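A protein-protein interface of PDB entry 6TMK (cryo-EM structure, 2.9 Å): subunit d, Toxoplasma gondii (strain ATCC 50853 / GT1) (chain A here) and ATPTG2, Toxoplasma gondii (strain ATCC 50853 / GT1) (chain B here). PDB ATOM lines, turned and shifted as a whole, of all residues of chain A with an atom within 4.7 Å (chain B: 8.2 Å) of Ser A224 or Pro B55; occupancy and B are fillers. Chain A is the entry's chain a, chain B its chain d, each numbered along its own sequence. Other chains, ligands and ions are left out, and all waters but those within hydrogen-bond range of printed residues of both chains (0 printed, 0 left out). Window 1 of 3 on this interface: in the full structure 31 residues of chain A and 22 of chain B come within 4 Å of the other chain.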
ATOM      1  N   LEU A 222      -5.581   4.732   7.213  1.00  0.00           N
ATOM      2  CA  LEU A 222      -5.440   4.381   5.813  1.00  0.00           C
ATOM      3  C   LEU A 222      -6.029   5.464   4.925  1.00  0.00           C
ATOM      4  O   LEU A 222      -6.894   6.233   5.352  1.00  0.00           O
ATOM      5  CB  LEU A 222      -6.134   3.056   5.532  1.00  0.00           C
ATOM      6  CG  LEU A 222      -5.667   1.856   6.341  1.00  0.00           C
ATOM      7  CD1 LEU A 222      -6.660   0.734   6.203  1.00  0.00           C
ATOM      8  CD2 LEU A 222      -4.309   1.423   5.862  1.00  0.00           C
ATOM      9  N   PRO A 223      -5.583   5.552   3.681  1.00  0.00           N
ATOM     10  CA  PRO A 223      -6.213   6.455   2.719  1.00  0.00           C
ATOM     11  C   PRO A 223      -7.502   5.863   2.162  1.00  0.00           C
ATOM     12  O   PRO A 223      -7.897   4.746   2.478  1.00  0.00           O
ATOM     13  CB  PRO A 223      -5.144   6.602   1.639  1.00  0.00           C
ATOM     14  CG  PRO A 223      -4.384   5.356   1.703  1.00  0.00           C
ATOM     15  CD  PRO A 223      -4.341   4.978   3.144  1.00  0.00           C
ATOM     16  N   SER A 224      -8.154   6.649   1.306  1.00  0.00           N
ATOM     17  CA  SER A 224      -9.478   6.294   0.811  1.00  0.00           C
ATOM     18  C   SER A 224      -9.456   4.982   0.038  1.00  0.00           C
ATOM     19  O   SER A 224     -10.265   4.080   0.290  1.00  0.00           O
ATOM     20  CB  SER A 224     -10.007   7.424  -0.067  1.00  0.00           C
ATOM     21  OG  SER A 224     -11.316   7.151  -0.529  1.00  0.00           O
ATOM     22  N   TRP A 225      -8.535   4.862  -0.916  1.00  0.00           N
ATOM     23  CA  TRP A 225      -8.524   3.708  -1.804  1.00  0.00           C
ATOM     24  C   TRP A 225      -8.266   2.421  -1.035  1.00  0.00           C
ATOM     25  O   TRP A 225      -9.004   1.441  -1.176  1.00  0.00           O
ATOM     26  CB  TRP A 225      -7.466   3.907  -2.885  1.00  0.00           C
ATOM     27  CG  TRP A 225      -7.643   3.048  -4.079  1.00  0.00           C
ATOM     28  CD1 TRP A 225      -8.256   3.385  -5.240  1.00  0.00           C
ATOM     29  CD2 TRP A 225      -7.197   1.701  -4.235  1.00  0.00           C
ATOM     30  NE1 TRP A 225      -8.224   2.333  -6.115  1.00  0.00           N
ATOM     31  CE2 TRP A 225      -7.578   1.284  -5.520  1.00  0.00           C
ATOM     32  CE3 TRP A 225      -6.514   0.806  -3.413  1.00  0.00           C
ATOM     33  CZ2 TRP A 225      -7.299   0.016  -6.001  1.00  0.00           C
ATOM     34  CZ3 TRP A 225      -6.239  -0.451  -3.893  1.00  0.00           C
ATOM     35  CH2 TRP A 225      -6.630  -0.836  -5.172  1.00  0.00           C
ATOM     36  N   GLU A 226      -7.218   2.406  -0.214  1.00  0.00           N
ATOM     37  CA  GLU A 226      -6.887   1.207   0.543  1.00  0.00           C
ATOM     38  C   GLU A 226      -7.961   0.901   1.577  1.00  0.00           C
ATOM     39  O   GLU A 226      -8.294  -0.268   1.810  1.00  0.00           O
ATOM     40  CB  GLU A 226      -5.530   1.377   1.211  1.00  0.00           C
ATOM     41  CG  GLU A 226      -4.391   1.646   0.247  1.00  0.00           C
ATOM     42  CD  GLU A 226      -3.986   0.422  -0.546  1.00  0.00           C
ATOM     43  OE1 GLU A 226      -4.626  -0.636  -0.382  1.00  0.00           O
ATOM     44  OE2 GLU A 226      -3.022   0.519  -1.336  1.00  0.00           O
ATOM     45  N   TYR A 227      -8.515   1.937   2.204  1.00  0.00           N
ATOM     46  CA  TYR A 227      -9.583   1.727   3.169  1.00  0.00           C
ATOM     47  C   TYR A 227     -10.762   1.020   2.524  1.00  0.00           C
ATOM     48  O   TYR A 227     -11.256   0.018   3.047  1.00  0.00           O
ATOM     49  CB  TYR A 227     -10.021   3.065   3.763  1.00  0.00           C
ATOM     50  CG  TYR A 227     -11.081   2.945   4.827  1.00  0.00           C
ATOM     51  CD1 TYR A 227     -10.739   2.836   6.163  1.00  0.00           C
ATOM     52  CD2 TYR A 227     -12.423   2.947   4.497  1.00  0.00           C
ATOM     53  CE1 TYR A 227     -11.704   2.725   7.134  1.00  0.00           C
ATOM     54  CE2 TYR A 227     -13.390   2.838   5.461  1.00  0.00           C
ATOM     55  CZ  TYR A 227     -13.027   2.725   6.778  1.00  0.00           C
ATOM     56  OH  TYR A 227     -13.994   2.618   7.747  1.00  0.00           O
ATOM     57  N   TYR A 228     -11.231   1.528   1.385  1.00  0.00           N
ATOM     58  CA  TYR A 228     -12.382   0.917   0.739  1.00  0.00           C
ATOM     59  C   TYR A 228     -12.046  -0.415   0.090  1.00  0.00           C
ATOM     60  O   TYR A 228     -12.947  -1.235  -0.112  1.00  0.00           O
ATOM     61  CB  TYR A 228     -12.962   1.859  -0.310  1.00  0.00           C
ATOM     62  CG  TYR A 228     -13.577   3.121   0.238  1.00  0.00           C
ATOM     63  CD1 TYR A 228     -14.484   3.080   1.278  1.00  0.00           C
ATOM     64  CD2 TYR A 228     -13.262   4.350  -0.301  1.00  0.00           C
ATOM     65  CE1 TYR A 228     -15.047   4.225   1.768  1.00  0.00           C
ATOM     66  CE2 TYR A 228     -13.821   5.500   0.185  1.00  0.00           C
ATOM     67  CZ  TYR A 228     -14.712   5.433   1.220  1.00  0.00           C
ATOM     68  OH  TYR A 228     -15.274   6.585   1.707  1.00  0.00           O
ATOM     69  N   HIS A 238     -20.964   3.889   2.668  1.00  0.00           N
ATOM     70  CA  HIS A 238     -20.573   5.247   2.314  1.00  0.00           C
ATOM     71  C   HIS A 238     -21.067   5.646   0.937  1.00  0.00           C
ATOM     72  O   HIS A 238     -21.200   6.842   0.660  1.00  0.00           O
ATOM     73  CB  HIS A 238     -19.054   5.387   2.368  1.00  0.00           C
ATOM     74  CG  HIS A 238     -18.477   5.229   3.737  1.00  0.00           C
ATOM     75  ND1 HIS A 238     -17.142   5.429   4.007  1.00  0.00           N
ATOM     76  CD2 HIS A 238     -19.051   4.890   4.914  1.00  0.00           C
ATOM     77  CE1 HIS A 238     -16.919   5.219   5.292  1.00  0.00           C
ATOM     78  NE2 HIS A 238     -18.062   4.892   5.864  1.00  0.00           N
ATOM     79  N   PRO A 254     -16.828  11.201  -3.402  1.00  0.00           N
ATOM     80  CA  PRO A 254     -15.733  11.953  -2.788  1.00  0.00           C
ATOM     81  C   PRO A 254     -14.599  11.059  -2.318  1.00  0.00           C
ATOM     82  O   PRO A 254     -14.791   9.888  -1.984  1.00  0.00           O
ATOM     83  CB  PRO A 254     -16.411  12.648  -1.602  1.00  0.00           C
ATOM     84  CG  PRO A 254     -17.566  11.800  -1.298  1.00  0.00           C
ATOM     85  CD  PRO A 254     -18.062  11.342  -2.618  1.00  0.00           C
ATOM     86  N   GLU A 255     -13.397  11.638  -2.296  1.00  0.00           N
ATOM     87  CA  GLU A 255     -12.229  10.906  -1.825  1.00  0.00           C
ATOM     88  C   GLU A 255     -12.393  10.499  -0.366  1.00  0.00           C
ATOM     89  O   GLU A 255     -12.270   9.320  -0.018  1.00  0.00           O
ATOM     90  CB  GLU A 255     -10.983  11.769  -2.011  1.00  0.00           C
ATOM     91  CG  GLU A 255      -9.676  11.009  -2.066  1.00  0.00           C
ATOM     92  CD  GLU A 255      -8.537  11.866  -2.575  1.00  0.00           C
ATOM     93  OE1 GLU A 255      -7.800  11.410  -3.472  1.00  0.00           O
ATOM     94  OE2 GLU A 255      -8.387  13.004  -2.086  1.00  0.00           O
ATOM     95  N   MET A 256     -12.678  11.470   0.503  1.00  0.00           N
ATOM     96  CA  MET A 256     -12.909  11.232   1.918  1.00  0.00           C
ATOM     97  C   MET A 256     -14.259  11.834   2.291  1.00  0.00           C
ATOM     98  O   MET A 256     -14.544  12.982   1.913  1.00  0.00           O
ATOM     99  CB  MET A 256     -11.790  11.836   2.781  1.00  0.00           C
ATOM    100  CG  MET A 256     -11.546  13.312   2.552  1.00  0.00           C
ATOM    101  SD  MET A 256     -10.231  13.978   3.590  1.00  0.00           S
ATOM    102  CE  MET A 256     -11.077  14.115   5.165  1.00  0.00           C
ATOM    103  N   PRO A 257     -15.117  11.114   3.010  1.00  0.00           N
ATOM    104  CA  PRO A 257     -16.440  11.650   3.317  1.00  0.00           C
ATOM    105  C   PRO A 257     -16.377  12.660   4.447  1.00  0.00           C
ATOM    106  O   PRO A 257     -15.375  12.735   5.173  1.00  0.00           O
ATOM    107  CB  PRO A 257     -17.242  10.406   3.728  1.00  0.00           C
ATOM    108  CG  PRO A 257     -16.368   9.249   3.452  1.00  0.00           C
ATOM    109  CD  PRO A 257     -14.982   9.744   3.515  1.00  0.00           C
ATOM    110  N   HIS B  51     -10.788   1.536  12.843  1.00  0.00           N
ATOM    111  CA  HIS B  51     -11.144   1.884  11.477  1.00  0.00           C
ATOM    112  C   HIS B  51     -12.633   2.132  11.311  1.00  0.00           C
ATOM    113  O   HIS B  51     -13.140   2.089  10.186  1.00  0.00           O
ATOM    114  CB  HIS B  51     -10.693   0.785  10.520  1.00  0.00           C
ATOM    115  CG  HIS B  51      -9.217   0.550  10.518  1.00  0.00           C
ATOM    116  ND1 HIS B  51      -8.301   1.576  10.438  1.00  0.00           N
ATOM    117  CD2 HIS B  51      -8.496  -0.594  10.573  1.00  0.00           C
ATOM    118  CE1 HIS B  51      -7.079   1.074  10.452  1.00  0.00           C
ATOM    119  NE2 HIS B  51      -7.170  -0.240  10.535  1.00  0.00           N
ATOM    120  N   ARG B  52     -13.347   2.388  12.406  1.00  0.00           N
ATOM    121  CA  ARG B  52     -14.789   2.554  12.303  1.00  0.00           C
ATOM    122  C   ARG B  52     -15.147   3.839  11.573  1.00  0.00           C
ATOM    123  O   ARG B  52     -16.070   3.857  10.751  1.00  0.00           O
ATOM    124  CB  ARG B  52     -15.413   2.541  13.697  1.00  0.00           C
ATOM    125  CG  ARG B  52     -16.926   2.639  13.707  1.00  0.00           C
ATOM    126  CD  ARG B  52     -17.564   1.459  13.013  1.00  0.00           C
ATOM    127  NE  ARG B  52     -17.721   1.698  11.583  1.00  0.00           N
ATOM    128  CZ  ARG B  52     -18.242   0.822  10.734  1.00  0.00           C
ATOM    129  NH1 ARG B  52     -18.664  -0.356  11.167  1.00  0.00           N
ATOM    130  NH2 ARG B  52     -18.345   1.126   9.450  1.00  0.00           N
ATOM    131  N   PHE B  53     -14.430   4.919  11.853  1.00  0.00           N
ATOM    132  CA  PHE B  53     -14.813   6.244  11.374  1.00  0.00           C
ATOM    133  C   PHE B  53     -14.068   6.598  10.089  1.00  0.00           C
ATOM    134  O   PHE B  53     -13.357   7.594   9.985  1.00  0.00           O
ATOM    135  CB  PHE B  53     -14.587   7.274  12.468  1.00  0.00           C
ATOM    136  CG  PHE B  53     -15.710   7.337  13.452  1.00  0.00           C
ATOM    137  CD1 PHE B  53     -16.871   8.019  13.148  1.00  0.00           C
ATOM    138  CD2 PHE B  53     -15.621   6.682  14.663  1.00  0.00           C
ATOM    139  CE1 PHE B  53     -17.910   8.066  14.045  1.00  0.00           C
ATOM    140  CE2 PHE B  53     -16.658   6.724  15.562  1.00  0.00           C
ATOM    141  CZ  PHE B  53     -17.804   7.417  15.252  1.00  0.00           C
ATOM    142  N   GLY B  54     -14.253   5.731   9.100  1.00  0.00           N
ATOM    143  CA  GLY B  54     -14.015   6.062   7.717  1.00  0.00           C
ATOM    144  C   GLY B  54     -12.605   6.501   7.404  1.00  0.00           C
ATOM    145  O   GLY B  54     -11.710   6.483   8.253  1.00  0.00           O
ATOM    146  N   PRO B  55     -12.388   6.899   6.151  1.00  0.00           N
ATOM    147  CA  PRO B  55     -11.113   7.515   5.766  1.00  0.00           C
ATOM    148  C   PRO B  55     -11.031   8.961   6.226  1.00  0.00           C
ATOM    149  O   PRO B  55     -11.932   9.762   5.968  1.00  0.00           O
ATOM    150  CB  PRO B  55     -11.126   7.428   4.236  1.00  0.00           C
ATOM    151  CG  PRO B  55     -12.195   6.471   3.898  1.00  0.00           C
ATOM    152  CD  PRO B  55     -13.209   6.597   4.974  1.00  0.00           C
ATOM    153  N   THR B  56      -9.944   9.289   6.916  1.00  0.00           N
ATOM    154  CA  THR B  56      -9.624  10.669   7.232  1.00  0.00           C
ATOM    155  C   THR B  56      -8.597  11.260   6.280  1.00  0.00           C
ATOM    156  O   THR B  56      -8.401  12.478   6.284  1.00  0.00           O
ATOM    157  CB  THR B  56      -9.102  10.771   8.668  1.00  0.00           C
ATOM    158  OG1 THR B  56      -7.729  10.365   8.709  1.00  0.00           O
ATOM    159  CG2 THR B  56      -9.910   9.875   9.580  1.00  0.00           C
ATOM    160  N   LEU B  57      -7.953  10.431   5.461  1.00  0.00           N
ATOM    161  CA  LEU B  57      -6.851  10.854   4.621  1.00  0.00           C
ATOM    162  C   LEU B  57      -7.186  10.661   3.150  1.00  0.00           C
ATOM    163  O   LEU B  57      -7.886   9.710   2.791  1.00  0.00           O
ATOM    164  CB  LEU B  57      -5.589  10.056   4.952  1.00  0.00           C
ATOM    165  CG  LEU B  57      -5.006  10.281   6.342  1.00  0.00           C
ATOM    166  CD1 LEU B  57      -3.899   9.294   6.584  1.00  0.00           C
ATOM    167  CD2 LEU B  57      -4.518  11.696   6.503  1.00  0.00           C
ATOM    168  N   PRO B  58      -6.701  11.531   2.277  1.00  0.00           N
ATOM    169  CA  PRO B  58      -6.861  11.318   0.840  1.00  0.00           C
ATOM    170  C   PRO B  58      -5.821  10.338   0.306  1.00  0.00           C
ATOM    171  O   PRO B  58      -5.014   9.780   1.043  1.00  0.00           O
ATOM    172  CB  PRO B  58      -6.668  12.721   0.271  1.00  0.00           C
ATOM    173  CG  PRO B  58      -5.732  13.353   1.203  1.00  0.00           C
ATOM    174  CD  PRO B  58      -6.133  12.858   2.558  1.00  0.00           C
ATOM    175  N   ASP B  59      -5.858  10.136  -1.010  1.00  0.00           N
ATOM    176  CA  ASP B  59      -4.960   9.176  -1.640  1.00  0.00           C
ATOM    177  C   ASP B  59      -3.560   9.741  -1.834  1.00  0.00           C
ATOM    178  O   ASP B  59      -2.568   9.039  -1.610  1.00  0.00           O
ATOM    179  CB  ASP B  59      -5.538   8.731  -2.979  1.00  0.00           C
ATOM    180  CG  ASP B  59      -6.787   7.897  -2.824  1.00  0.00           C
ATOM    181  OD1 ASP B  59      -6.812   7.023  -1.935  1.00  0.00           O
ATOM    182  OD2 ASP B  59      -7.747   8.116  -3.591  1.00  0.00           O
ATOM    183  N   HIS B  60      -3.458  11.005  -2.246  1.00  0.00           N
ATOM    184  CA  HIS B  60      -2.150  11.609  -2.462  1.00  0.00           C
ATOM    185  C   HIS B  60      -1.352  11.733  -1.174  1.00  0.00           C
ATOM    186  O   HIS B  60      -0.133  11.917  -1.228  1.00  0.00           O
ATOM    187  CB  HIS B  60      -2.303  12.977  -3.119  1.00  0.00           C
ATOM    188  CG  HIS B  60      -2.878  14.023  -2.218  1.00  0.00           C
ATOM    189  ND1 HIS B  60      -2.111  14.736  -1.323  1.00  0.00           N
ATOM    190  CD2 HIS B  60      -4.141  14.486  -2.085  1.00  0.00           C
ATOM    191  CE1 HIS B  60      -2.880  15.587  -0.671  1.00  0.00           C
ATOM    192  NE2 HIS B  60      -4.117  15.454  -1.113  1.00  0.00           N
ATOM    193  N   ALA B  61      -2.011  11.647  -0.020  1.00  0.00           N
ATOM    194  CA  ALA B  61      -1.285  11.597   1.239  1.00  0.00           C
ATOM    195  C   ALA B  61      -0.417  10.355   1.349  1.00  0.00           C
ATOM    196  O   ALA B  61       0.567  10.363   2.094  1.00  0.00           O
ATOM    197  CB  ALA B  61      -2.265  11.644   2.404  1.00  0.00           C
ATOM    198  N   TYR B  62      -0.763   9.288   0.635  1.00  0.00           N
ATOM    199  CA  TYR B  62      -0.028   8.034   0.686  1.00  0.00           C
ATOM    200  C   TYR B  62       0.751   7.758  -0.588  1.00  0.00           C
ATOM    201  O   TYR B  62       1.931   7.403  -0.532  1.00  0.00           O
ATOM    202  CB  TYR B  62      -0.981   6.864   0.949  1.00  0.00           C
ATOM    203  CG  TYR B  62      -0.355   5.535   0.625  1.00  0.00           C
ATOM    204  CD1 TYR B  62       0.631   5.002   1.431  1.00  0.00           C
ATOM    205  CD2 TYR B  62      -0.731   4.826  -0.497  1.00  0.00           C
ATOM    206  CE1 TYR B  62       1.216   3.795   1.133  1.00  0.00           C
ATOM    207  CE2 TYR B  62      -0.151   3.623  -0.802  1.00  0.00           C
ATOM    208  CZ  TYR B  62       0.824   3.113   0.013  1.00  0.00           C
ATOM    209  OH  TYR B  62       1.402   1.909  -0.292  1.00  0.00           O
ATOM    210  N   TYR B  63       0.114   7.914  -1.742  1.00  0.00           N
ATOM    211  CA  TYR B  63       0.680   7.399  -2.978  1.00  0.00           C
ATOM    212  C   TYR B  63       1.840   8.258  -3.452  1.00  0.00           C
ATOM    213  O   TYR B  63       1.835   9.483  -3.306  1.00  0.00           O
ATOM    214  CB  TYR B  63      -0.390   7.336  -4.060  1.00  0.00           C
ATOM    215  CG  TYR B  63      -1.354   6.198  -3.881  1.00  0.00           C
ATOM    216  CD1 TYR B  63      -0.957   4.894  -4.094  1.00  0.00           C
ATOM    217  CD2 TYR B  63      -2.656   6.427  -3.487  1.00  0.00           C
ATOM    218  CE1 TYR B  63      -1.831   3.851  -3.923  1.00  0.00           C
ATOM    219  CE2 TYR B  63      -3.538   5.392  -3.314  1.00  0.00           C
ATOM    220  CZ  TYR B  63      -3.120   4.104  -3.535  1.00  0.00           C
ATOM    221  OH  TYR B  63      -3.987   3.058  -3.365  1.00  0.00           O
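Of the 13 printed residues of chain B, 10 touch a printed residue of chain A. Printed residues of chain B that touch a printed residue of chain A: His B51, Arg B52, Gly B54, Pro B55, Thr B56, Leu B57, Pro B58, Asp B59, Tyr B62 and Tyr B63. Printed residues of chain A that touch a printed residue of chain B: Pro A223, Ser A224, Trp A225, Glu A226, Tyr A227, Tyr A228, His A238, Glu A255, Met A256 and Pro A257. Hydrophobic or aromatic side chains of chain A that line the printed part of chain B: Pro A223, Trp A225, Tyr A227, Tyr A228, His A238, Met A256 and Pro A257. Along chain A the printed residues that touch a printed residue of chain B span positions 223 to 257.
The backbone NH (N) of Gly B54 is in hydrogen-bond range of the side-chain hydroxyl (OH) of Tyr A227. The side-chain carboxylate (OE2) of Glu A226 lies within hydrogen-bond range of the side-chain hydroxyl (OH) of Tyr B63 (3.4 Å). The backbone NH of Ser A224 is in hydrogen-bond range of the backbone carbonyl oxygen of Leu B57 (3.4 Å). The side-chain carboxylate (OE1) of Glu A255 is in hydrogen-bond range of the backbone NH (N) of Asp B59, 3.4 Å away. The side-chain hydroxyl (OH) of Tyr A227 sits at hydrogen-bond distance from the backbone carbonyl oxygen (O) of His B51 (2.6 Å). The side-chain carboxylate (OD1) of Asp B59 is in hydrogen-bond range of the backbone NH (N) of Trp A225 (2.9 Å). O of Thr B56 sits close to SD of Met A256.
Pro A223 touches Pro B58. CB of Pro A223 touches OD1 of Asp B59 (3.97 Å). CB of Tyr B62 touches CG of Pro A223 (3.8 Å). CA of Ser A224 touches CB of Pro B55, 3.97 Å away. Asp B59 touches Ser A224. Tyr A227 touches Pro B55. His A238 touches Gly B54. CD of Pro B55 touches CE1 of His A238 (3.97 Å). Glu A255 touches Pro B58 (OE2 to CB, 2.9 Å). Pro A257 touches Pro B55 (CD to CD, 3.9 Å).
The side-chain hydroxyl of Tyr A228 is in hydrogen-bond range of a ring nitrogen (ND1) of His A238 (3.2 Å). The side-chain hydroxyl (OG) of Ser A224 lies within hydrogen-bond range of the backbone carbonyl oxygen (O) of Glu A255, at 2.4 Å.
Ser A224 touches just these residues of chain B: Pro B55 (3.97 Å), Leu B57 (3.4 Å) and Asp B59 (3.5 Å). Printed residues of chain B within 4 Å of His A238: Gly B54 (3.9 Å) and Pro B55 (3.97 Å). Pro B55 touches just these residues of chain A: Ser A224, Tyr A227, Tyr A228, His A238, Met A256 and Pro A257. Of the printed residues of chain A, Asp B59 touches Pro A223 (3.97 Å), Ser A224 (3.5 Å), Trp A225 (2.9 Å) and Glu A255 (3.3 Å). His B60 touches none of the printed residues of chain A. Ala B61 touches none of the printed residues of chain A. Of the printed residues of chain A, Tyr B62 touches Pro A223. Of the printed residues of chain A, Tyr B63 touches Trp A225 (3.4 Å) and Glu A226 (3.4 Å). The nearest residue of chain B that does not touch Ser A224 is Pro B58 (4.4 Å). The nearest printed residue of chain B that does not touch Pro A257 is Gly B54 (5.6 Å).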
